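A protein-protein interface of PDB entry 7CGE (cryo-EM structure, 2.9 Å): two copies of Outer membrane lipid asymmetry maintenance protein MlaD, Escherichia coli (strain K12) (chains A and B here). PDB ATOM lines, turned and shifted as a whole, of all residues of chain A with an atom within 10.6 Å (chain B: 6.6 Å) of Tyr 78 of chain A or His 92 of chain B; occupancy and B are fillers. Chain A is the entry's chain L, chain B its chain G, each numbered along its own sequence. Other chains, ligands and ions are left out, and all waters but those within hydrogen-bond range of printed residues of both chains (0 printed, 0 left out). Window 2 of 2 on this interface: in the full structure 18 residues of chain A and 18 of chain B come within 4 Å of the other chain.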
ATOM      1  N   THR A  45     -13.847  26.325   5.513  1.00  0.00           N
ATOM      2  CA  THR A  45     -14.191  25.480   6.647  1.00  0.00           C
ATOM      3  C   THR A  45     -13.426  24.171   6.533  1.00  0.00           C
ATOM      4  O   THR A  45     -13.522  23.482   5.514  1.00  0.00           O
ATOM      5  CB  THR A  45     -15.696  25.222   6.698  1.00  0.00           C
ATOM      6  OG1 THR A  45     -16.383  26.474   6.783  1.00  0.00           O
ATOM      7  CG2 THR A  45     -16.053  24.394   7.908  1.00  0.00           C
ATOM      8  N   PHE A  46     -12.680  23.832   7.573  1.00  0.00           N
ATOM      9  CA  PHE A  46     -11.859  22.634   7.616  1.00  0.00           C
ATOM     10  C   PHE A  46     -12.466  21.643   8.596  1.00  0.00           C
ATOM     11  O   PHE A  46     -13.545  21.859   9.145  1.00  0.00           O
ATOM     12  CB  PHE A  46     -10.425  22.971   8.026  1.00  0.00           C
ATOM     13  CG  PHE A  46      -9.695  23.830   7.048  1.00  0.00           C
ATOM     14  CD1 PHE A  46      -9.790  25.205   7.108  1.00  0.00           C
ATOM     15  CD2 PHE A  46      -8.893  23.265   6.086  1.00  0.00           C
ATOM     16  CE1 PHE A  46      -9.121  25.992   6.215  1.00  0.00           C
ATOM     17  CE2 PHE A  46      -8.216  24.054   5.195  1.00  0.00           C
ATOM     18  CZ  PHE A  46      -8.335  25.418   5.261  1.00  0.00           C
ATOM     19  N   ASP A  47     -11.753  20.541   8.815  1.00  0.00           N
ATOM     20  CA  ASP A  47     -12.037  19.630   9.917  1.00  0.00           C
ATOM     21  C   ASP A  47     -11.087  19.846  11.084  1.00  0.00           C
ATOM     22  O   ASP A  47     -11.524  19.981  12.228  1.00  0.00           O
ATOM     23  CB  ASP A  47     -11.943  18.179   9.446  1.00  0.00           C
ATOM     24  CG  ASP A  47     -13.037  17.810   8.486  1.00  0.00           C
ATOM     25  OD1 ASP A  47     -14.134  18.396   8.581  1.00  0.00           O
ATOM     26  OD2 ASP A  47     -12.802  16.928   7.636  1.00  0.00           O
ATOM     27  N   ASN A  48      -9.787  19.881  10.804  1.00  0.00           N
ATOM     28  CA  ASN A  48      -8.753  20.141  11.793  1.00  0.00           C
ATOM     29  C   ASN A  48      -7.793  21.165  11.219  1.00  0.00           C
ATOM     30  O   ASN A  48      -7.336  21.015  10.082  1.00  0.00           O
ATOM     31  CB  ASN A  48      -8.001  18.864  12.154  1.00  0.00           C
ATOM     32  CG  ASN A  48      -7.008  19.074  13.261  1.00  0.00           C
ATOM     33  OD1 ASN A  48      -7.268  19.802  14.212  1.00  0.00           O
ATOM     34  ND2 ASN A  48      -5.858  18.436  13.146  1.00  0.00           N
ATOM     35  N   ILE A  49      -7.486  22.201  11.995  1.00  0.00           N
ATOM     36  CA  ILE A  49      -6.590  23.257  11.550  1.00  0.00           C
ATOM     37  C   ILE A  49      -5.319  23.329  12.365  1.00  0.00           C
ATOM     38  O   ILE A  49      -4.467  24.172  12.064  1.00  0.00           O
ATOM     39  CB  ILE A  49      -7.273  24.634  11.582  1.00  0.00           C
ATOM     40  CG1 ILE A  49      -7.530  25.023  13.026  1.00  0.00           C
ATOM     41  CG2 ILE A  49      -8.554  24.616  10.804  1.00  0.00           C
ATOM     42  CD1 ILE A  49      -7.763  26.448  13.198  1.00  0.00           C
ATOM     43  N   THR A  72     -12.713  31.118  14.305  1.00  0.00           N
ATOM     44  CA  THR A  72     -13.797  31.436  15.227  1.00  0.00           C
ATOM     45  C   THR A  72     -14.466  30.206  15.841  1.00  0.00           C
ATOM     46  O   THR A  72     -15.029  30.314  16.938  1.00  0.00           O
ATOM     47  CB  THR A  72     -14.828  32.339  14.535  1.00  0.00           C
ATOM     48  OG1 THR A  72     -15.635  32.979  15.527  1.00  0.00           O
ATOM     49  CG2 THR A  72     -15.734  31.567  13.591  1.00  0.00           C
ATOM     50  N   LEU A  73     -14.391  29.035  15.179  1.00  0.00           N
ATOM     51  CA  LEU A  73     -15.083  27.803  15.589  1.00  0.00           C
ATOM     52  C   LEU A  73     -16.583  28.037  15.716  1.00  0.00           C
ATOM     53  O   LEU A  73     -17.092  28.224  16.826  1.00  0.00           O
ATOM     54  CB  LEU A  73     -14.522  27.202  16.888  1.00  0.00           C
ATOM     55  CG  LEU A  73     -15.041  25.829  17.354  1.00  0.00           C
ATOM     56  CD1 LEU A  73     -15.054  24.801  16.239  1.00  0.00           C
ATOM     57  CD2 LEU A  73     -14.261  25.330  18.547  1.00  0.00           C
ATOM     58  N   ASP A  74     -17.263  28.182  14.589  1.00  0.00           N
ATOM     59  CA  ASP A  74     -18.701  28.412  14.543  1.00  0.00           C
ATOM     60  C   ASP A  74     -19.481  27.315  15.260  1.00  0.00           C
ATOM     61  O   ASP A  74     -19.051  26.157  15.273  1.00  0.00           O
ATOM     62  CB  ASP A  74     -19.161  28.522  13.088  1.00  0.00           C
ATOM     63  CG  ASP A  74     -19.037  27.215  12.335  1.00  0.00           C
ATOM     64  OD1 ASP A  74     -17.962  26.965  11.766  1.00  0.00           O
ATOM     65  OD2 ASP A  74     -20.011  26.437  12.299  1.00  0.00           O
ATOM     66  N   PRO A  75     -20.636  27.634  15.861  1.00  0.00           N
ATOM     67  CA  PRO A  75     -21.452  26.595  16.506  1.00  0.00           C
ATOM     68  C   PRO A  75     -22.204  25.731  15.512  1.00  0.00           C
ATOM     69  O   PRO A  75     -21.846  25.692  14.329  1.00  0.00           O
ATOM     70  CB  PRO A  75     -22.413  27.402  17.384  1.00  0.00           C
ATOM     71  CG  PRO A  75     -22.535  28.702  16.686  1.00  0.00           C
ATOM     72  CD  PRO A  75     -21.197  28.981  16.073  1.00  0.00           C
ATOM     73  N   LYS A  76     -23.128  24.911  16.028  1.00  0.00           N
ATOM     74  CA  LYS A  76     -24.184  24.201  15.295  1.00  0.00           C
ATOM     75  C   LYS A  76     -23.662  23.006  14.490  1.00  0.00           C
ATOM     76  O   LYS A  76     -24.416  22.075  14.190  1.00  0.00           O
ATOM     77  CB  LYS A  76     -24.914  25.213  14.380  1.00  0.00           C
ATOM     78  CG  LYS A  76     -25.936  24.722  13.368  1.00  0.00           C
ATOM     79  CD  LYS A  76     -26.098  25.764  12.257  1.00  0.00           C
ATOM     80  CE  LYS A  76     -26.493  27.145  12.758  1.00  0.00           C
ATOM     81  NZ  LYS A  76     -27.940  27.424  12.539  1.00  0.00           N
ATOM     82  N   THR A  77     -22.359  22.953  14.231  1.00  0.00           N
ATOM     83  CA  THR A  77     -21.746  21.780  13.629  1.00  0.00           C
ATOM     84  C   THR A  77     -20.389  21.459  14.228  1.00  0.00           C
ATOM     85  O   THR A  77     -19.871  20.362  13.987  1.00  0.00           O
ATOM     86  CB  THR A  77     -21.611  21.959  12.116  1.00  0.00           C
ATOM     87  OG1 THR A  77     -21.025  20.782  11.545  1.00  0.00           O
ATOM     88  CG2 THR A  77     -20.766  23.184  11.790  1.00  0.00           C
ATOM     89  N   TYR A  78     -19.817  22.398  14.988  1.00  0.00           N
ATOM     90  CA  TYR A  78     -18.504  22.314  15.618  1.00  0.00           C
ATOM     91  C   TYR A  78     -17.396  22.018  14.617  1.00  0.00           C
ATOM     92  O   TYR A  78     -16.694  21.011  14.727  1.00  0.00           O
ATOM     93  CB  TYR A  78     -18.517  21.285  16.746  1.00  0.00           C
ATOM     94  CG  TYR A  78     -19.163  21.817  17.996  1.00  0.00           C
ATOM     95  CD1 TYR A  78     -18.750  23.022  18.548  1.00  0.00           C
ATOM     96  CD2 TYR A  78     -20.191  21.126  18.616  1.00  0.00           C
ATOM     97  CE1 TYR A  78     -19.339  23.518  19.690  1.00  0.00           C
ATOM     98  CE2 TYR A  78     -20.786  21.615  19.753  1.00  0.00           C
ATOM     99  CZ  TYR A  78     -20.357  22.808  20.285  1.00  0.00           C
ATOM    100  OH  TYR A  78     -20.955  23.289  21.421  1.00  0.00           O
ATOM    101  N   LEU A  79     -17.238  22.901  13.639  1.00  0.00           N
ATOM    102  CA  LEU A  79     -16.131  22.863  12.699  1.00  0.00           C
ATOM    103  C   LEU A  79     -15.450  24.220  12.732  1.00  0.00           C
ATOM    104  O   LEU A  79     -16.089  25.224  13.056  1.00  0.00           O
ATOM    105  CB  LEU A  79     -16.620  22.532  11.282  1.00  0.00           C
ATOM    106  CG  LEU A  79     -17.189  21.132  11.075  1.00  0.00           C
ATOM    107  CD1 LEU A  79     -17.502  20.905   9.619  1.00  0.00           C
ATOM    108  CD2 LEU A  79     -16.227  20.086  11.570  1.00  0.00           C
ATOM    109  N   PRO A  80     -14.152  24.285  12.447  1.00  0.00           N
ATOM    110  CA  PRO A  80     -13.473  25.580  12.427  1.00  0.00           C
ATOM    111  C   PRO A  80     -13.697  26.324  11.122  1.00  0.00           C
ATOM    112  O   PRO A  80     -13.757  25.743  10.039  1.00  0.00           O
ATOM    113  CB  PRO A  80     -11.995  25.202  12.593  1.00  0.00           C
ATOM    114  CG  PRO A  80     -11.985  23.761  12.944  1.00  0.00           C
ATOM    115  CD  PRO A  80     -13.188  23.185  12.320  1.00  0.00           C
ATOM    116  N   ARG A  81     -13.813  27.646  11.243  1.00  0.00           N
ATOM    117  CA  ARG A  81     -14.068  28.524  10.107  1.00  0.00           C
ATOM    118  C   ARG A  81     -12.971  29.575  10.049  1.00  0.00           C
ATOM    119  O   ARG A  81     -12.700  30.245  11.048  1.00  0.00           O
ATOM    120  CB  ARG A  81     -15.440  29.177  10.225  1.00  0.00           C
ATOM    121  CG  ARG A  81     -15.976  29.735   8.933  1.00  0.00           C
ATOM    122  CD  ARG A  81     -17.452  30.011   9.060  1.00  0.00           C
ATOM    123  NE  ARG A  81     -18.046  30.429   7.797  1.00  0.00           N
ATOM    124  CZ  ARG A  81     -18.167  31.695   7.418  1.00  0.00           C
ATOM    125  NH1 ARG A  81     -17.729  32.668   8.203  1.00  0.00           N
ATOM    126  NH2 ARG A  81     -18.722  31.985   6.251  1.00  0.00           N
ATOM    127  N   TYR B  40     -17.301  25.715  32.899  1.00  0.00           N
ATOM    128  CA  TYR B  40     -17.809  24.581  33.648  1.00  0.00           C
ATOM    129  C   TYR B  40     -16.816  23.429  33.569  1.00  0.00           C
ATOM    130  O   TYR B  40     -15.832  23.483  32.831  1.00  0.00           O
ATOM    131  CB  TYR B  40     -19.193  24.165  33.170  1.00  0.00           C
ATOM    132  CG  TYR B  40     -19.253  23.531  31.816  1.00  0.00           C
ATOM    133  CD1 TYR B  40     -19.260  24.303  30.673  1.00  0.00           C
ATOM    134  CD2 TYR B  40     -19.361  22.159  31.683  1.00  0.00           C
ATOM    135  CE1 TYR B  40     -19.347  23.719  29.427  1.00  0.00           C
ATOM    136  CE2 TYR B  40     -19.447  21.572  30.450  1.00  0.00           C
ATOM    137  CZ  TYR B  40     -19.444  22.351  29.327  1.00  0.00           C
ATOM    138  OH  TYR B  40     -19.532  21.753  28.097  1.00  0.00           O
ATOM    139  N   ILE B  60     -10.915  21.814  20.243  1.00  0.00           N
ATOM    140  CA  ILE B  60     -11.792  21.113  19.315  1.00  0.00           C
ATOM    141  C   ILE B  60     -11.405  21.568  17.920  1.00  0.00           C
ATOM    142  O   ILE B  60     -11.546  22.749  17.586  1.00  0.00           O
ATOM    143  CB  ILE B  60     -13.274  21.390  19.586  1.00  0.00           C
ATOM    144  CG1 ILE B  60     -13.583  21.260  21.070  1.00  0.00           C
ATOM    145  CG2 ILE B  60     -14.135  20.445  18.774  1.00  0.00           C
ATOM    146  CD1 ILE B  60     -14.993  21.615  21.408  1.00  0.00           C
ATOM    147  N   GLY B  61     -10.880  20.649  17.116  1.00  0.00           N
ATOM    148  CA  GLY B  61     -10.465  20.961  15.765  1.00  0.00           C
ATOM    149  C   GLY B  61      -9.266  21.873  15.636  1.00  0.00           C
ATOM    150  O   GLY B  61      -8.910  22.234  14.511  1.00  0.00           O
ATOM    151  N   ARG B  89     -19.830  28.690  26.306  1.00  0.00           N
ATOM    152  CA  ARG B  89     -20.308  28.937  24.953  1.00  0.00           C
ATOM    153  C   ARG B  89     -20.574  27.635  24.208  1.00  0.00           C
ATOM    154  O   ARG B  89     -21.476  27.574  23.367  1.00  0.00           O
ATOM    155  CB  ARG B  89     -19.289  29.800  24.214  1.00  0.00           C
ATOM    156  CG  ARG B  89     -19.731  30.311  22.866  1.00  0.00           C
ATOM    157  CD  ARG B  89     -19.232  31.724  22.624  1.00  0.00           C
ATOM    158  NE  ARG B  89     -17.776  31.817  22.546  1.00  0.00           N
ATOM    159  CZ  ARG B  89     -17.011  32.406  23.460  1.00  0.00           C
ATOM    160  NH1 ARG B  89     -17.558  32.949  24.538  1.00  0.00           N
ATOM    161  NH2 ARG B  89     -15.697  32.448  23.299  1.00  0.00           N
ATOM    162  N   TYR B  90     -19.814  26.590  24.504  1.00  0.00           N
ATOM    163  CA  TYR B  90     -19.906  25.324  23.779  1.00  0.00           C
ATOM    164  C   TYR B  90     -20.681  24.283  24.585  1.00  0.00           C
ATOM    165  O   TYR B  90     -20.165  23.233  24.954  1.00  0.00           O
ATOM    166  CB  TYR B  90     -18.506  24.831  23.414  1.00  0.00           C
ATOM    167  CG  TYR B  90     -17.620  25.935  22.873  1.00  0.00           C
ATOM    168  CD1 TYR B  90     -17.701  26.325  21.544  1.00  0.00           C
ATOM    169  CD2 TYR B  90     -16.719  26.603  23.695  1.00  0.00           C
ATOM    170  CE1 TYR B  90     -16.911  27.341  21.051  1.00  0.00           C
ATOM    171  CE2 TYR B  90     -15.931  27.620  23.209  1.00  0.00           C
ATOM    172  CZ  TYR B  90     -16.030  27.980  21.890  1.00  0.00           C
ATOM    173  OH  TYR B  90     -15.238  28.992  21.410  1.00  0.00           O
ATOM    174  N   ASN B  91     -21.950  24.579  24.847  1.00  0.00           N
ATOM    175  CA  ASN B  91     -22.790  23.695  25.654  1.00  0.00           C
ATOM    176  C   ASN B  91     -23.606  22.736  24.796  1.00  0.00           C
ATOM    177  O   ASN B  91     -24.824  22.665  24.917  1.00  0.00           O
ATOM    178  CB  ASN B  91     -23.706  24.525  26.539  1.00  0.00           C
ATOM    179  CG  ASN B  91     -22.958  25.222  27.640  1.00  0.00           C
ATOM    180  OD1 ASN B  91     -21.745  25.074  27.768  1.00  0.00           O
ATOM    181  ND2 ASN B  91     -23.672  26.001  28.442  1.00  0.00           N
ATOM    182  N   HIS B  92     -22.952  21.997  23.904  1.00  0.00           N
ATOM    183  CA  HIS B  92     -23.692  21.052  23.077  1.00  0.00           C
ATOM    184  C   HIS B  92     -22.859  19.797  22.817  1.00  0.00           C
ATOM    185  O   HIS B  92     -23.075  19.105  21.819  1.00  0.00           O
ATOM    186  CB  HIS B  92     -24.140  21.764  21.775  1.00  0.00           C
ATOM    187  CG  HIS B  92     -25.154  21.013  20.962  1.00  0.00           C
ATOM    188  ND1 HIS B  92     -26.447  20.802  21.387  1.00  0.00           N
ATOM    189  CD2 HIS B  92     -25.063  20.434  19.742  1.00  0.00           C
ATOM    190  CE1 HIS B  92     -27.105  20.116  20.471  1.00  0.00           C
ATOM    191  NE2 HIS B  92     -26.287  19.880  19.461  1.00  0.00           N
ATOM    192  N   ILE B  93     -21.913  19.477  23.688  1.00  0.00           N
ATOM    193  CA  ILE B  93     -21.007  18.364  23.429  1.00  0.00           C
ATOM    194  C   ILE B  93     -21.718  17.047  23.712  1.00  0.00           C
ATOM    195  O   ILE B  93     -22.168  16.824  24.841  1.00  0.00           O
ATOM    196  CB  ILE B  93     -19.727  18.490  24.265  1.00  0.00           C
ATOM    197  CG1 ILE B  93     -19.234  19.937  24.261  1.00  0.00           C
ATOM    198  CG2 ILE B  93     -18.658  17.547  23.745  1.00  0.00           C
ATOM    199  CD1 ILE B  93     -18.209  20.229  25.331  1.00  0.00           C
ATOM    200  N   PRO B  94     -21.846  16.159  22.727  1.00  0.00           N
ATOM    201  CA  PRO B  94     -22.442  14.847  22.993  1.00  0.00           C
ATOM    202  C   PRO B  94     -21.502  13.986  23.813  1.00  0.00           C
ATOM    203  O   PRO B  94     -20.281  14.069  23.669  1.00  0.00           O
ATOM    204  CB  PRO B  94     -22.644  14.259  21.593  1.00  0.00           C
ATOM    205  CG  PRO B  94     -22.481  15.409  20.655  1.00  0.00           C
ATOM    206  CD  PRO B  94     -21.509  16.321  21.309  1.00  0.00           C
ATOM    207  N   VAL B 116     -15.332  15.614  19.047  1.00  0.00           N
ATOM    208  CA  VAL B 116     -16.767  15.705  19.274  1.00  0.00           C
ATOM    209  C   VAL B 116     -17.455  14.556  18.552  1.00  0.00           C
ATOM    210  O   VAL B 116     -17.310  14.396  17.336  1.00  0.00           O
ATOM    211  CB  VAL B 116     -17.311  17.066  18.809  1.00  0.00           C
ATOM    212  CG1 VAL B 116     -18.820  17.024  18.659  1.00  0.00           C
ATOM    213  CG2 VAL B 116     -16.925  18.135  19.797  1.00  0.00           C
ATOM    214  N   PHE B 118     -20.172  13.808  16.975  1.00  0.00           N
ATOM    215  CA  PHE B 118     -21.278  14.537  16.350  1.00  0.00           C
ATOM    216  C   PHE B 118     -22.268  13.523  15.782  1.00  0.00           C
ATOM    217  O   PHE B 118     -22.296  13.216  14.589  1.00  0.00           O
ATOM    218  CB  PHE B 118     -20.726  15.497  15.290  1.00  0.00           C
ATOM    219  CG  PHE B 118     -21.775  16.294  14.544  1.00  0.00           C
ATOM    220  CD1 PHE B 118     -22.369  17.399  15.133  1.00  0.00           C
ATOM    221  CD2 PHE B 118     -22.086  16.003  13.219  1.00  0.00           C
ATOM    222  CE1 PHE B 118     -23.316  18.147  14.446  1.00  0.00           C
ATOM    223  CE2 PHE B 118     -23.031  16.746  12.527  1.00  0.00           C
ATOM    224  CZ  PHE B 118     -23.641  17.819  13.139  1.00  0.00           C
ATOM    225  N   ASP B 120     -25.574  12.487  18.169  1.00  0.00           N
ATOM    226  CA  ASP B 120     -26.828  12.573  18.915  1.00  0.00           C
ATOM    227  C   ASP B 120     -28.019  11.876  18.243  1.00  0.00           C
ATOM    228  O   ASP B 120     -29.090  12.470  18.100  1.00  0.00           O
ATOM    229  CB  ASP B 120     -27.157  14.036  19.191  1.00  0.00           C
ATOM    230  CG  ASP B 120     -28.064  14.226  20.400  1.00  0.00           C
ATOM    231  OD1 ASP B 120     -28.429  13.221  21.047  1.00  0.00           O
ATOM    232  OD2 ASP B 120     -28.416  15.387  20.701  1.00  0.00           O
ATOM    233  N   ALA B 126     -26.935  12.681  26.240  1.00  0.00           N
ATOM    234  CA  ALA B 126     -26.909  13.806  27.156  1.00  0.00           C
ATOM    235  C   ALA B 126     -25.854  14.834  26.753  1.00  0.00           C
ATOM    236  O   ALA B 126     -25.059  14.634  25.833  1.00  0.00           O
ATOM    237  CB  ALA B 126     -26.665  13.320  28.585  1.00  0.00           C
ATOM    238  N   ILE B 127     -25.872  15.957  27.459  1.00  0.00           N
ATOM    239  CA  ILE B 127     -24.940  17.053  27.246  1.00  0.00           C
ATOM    240  C   ILE B 127     -23.999  17.097  28.439  1.00  0.00           C
ATOM    241  O   ILE B 127     -24.443  17.001  29.589  1.00  0.00           O
ATOM    242  CB  ILE B 127     -25.684  18.388  27.063  1.00  0.00           C
ATOM    243  CG1 ILE B 127     -26.626  18.294  25.865  1.00  0.00           C
ATOM    244  CG2 ILE B 127     -24.724  19.560  26.894  1.00  0.00           C
ATOM    245  CD1 ILE B 127     -25.929  17.957  24.575  1.00  0.00           C
ATOM    246  N   LEU B 128     -22.702  17.207  28.161  1.00  0.00           N
ATOM    247  CA  LEU B 128     -21.716  17.416  29.207  1.00  0.00           C
ATOM    248  C   LEU B 128     -21.982  18.753  29.889  1.00  0.00           C
ATOM    249  O   LEU B 128     -21.815  19.819  29.288  1.00  0.00           O
ATOM    250  CB  LEU B 128     -20.299  17.353  28.626  1.00  0.00           C
ATOM    251  CG  LEU B 128     -19.781  15.939  28.332  1.00  0.00           C
ATOM    252  CD1 LEU B 128     -18.584  15.903  27.380  1.00  0.00           C
ATOM    253  CD2 LEU B 128     -19.410  15.273  29.633  1.00  0.00           C
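OH of Tyr 78 of chain A lies within hydrogen-bond range of N of His 92 of chain B (3.4 Å). OD1 of Asn 48 of chain A lies close to O of Gly 61 of chain B (2.9 Å). N of Ile 49 of chain A is in hydrogen-bond range of O of Gly 61 of chain B.
The backbone NH (N) of Phe 46 of chain A lies within hydrogen-bond range of the backbone carbonyl oxygen (O) of Pro 80 of chain A (3.3 Å).
Gly 61 of chain B touches Asp 47 of chain A (CA to O, 3.8 Å). Ile 60 of chain B touches Leu 73 of chain A (O to CD2, 3.9 Å). Tyr 78 of chain A touches Tyr 90 of chain B (OH to CA, 3.3 Å). Tyr 78 of chain A touches Asn 91 of chain B (OH to N, 3.8 Å). CG of Pro 80 of chain A touches O of Gly 61 of chain B, 3.8 Å away.
His 92 of chain B touches just one residue of chain A: Tyr 78. Of chain A, only Tyr 78 comes within 4 Å of Asn 91 of chain B. No residue of chain A comes within 4 Å of Ile 93 of chain B. Of the printed residues of chain B, Asp 47 of chain A touches Gly 61 (3.8 Å). Printed residues of chain A within 4 Å of Tyr 90 of chain B: Tyr 78. Of the printed residues of chain B, Asn 48 of chain A touches Gly 61. Printed residues of chain A within 4 Å of Ile 60 of chain B: Leu 73 (3.9 Å). Ile 127 of chain B touches none of the printed residues of chain A. The nearest residue of chain B that does not touch Tyr 78 of chain A is Val 116 of chain B (4.3 Å). The nearest printed residue of chain A that does not touch Tyr 90 of chain B is Leu 73 of chain A (4.2 Å).
Hydrophobic or aromatic side chains of chain B that line the printed part of chain A: Tyr 90 and His 92. Of the 15 printed residues of chain A, 6 touch a printed residue of chain B. Among the printed residues, 8 pairs touch across the chains. Among the printed residues, no Asp or Glu carboxylate lies within 4 Å of a Lys or Arg side-chain nitrogen of the other chain.
No position is printed for both chains. Of the 8 pairs that touch across the chains among the printed residues, none has its exchanged pair printed and touching as well.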
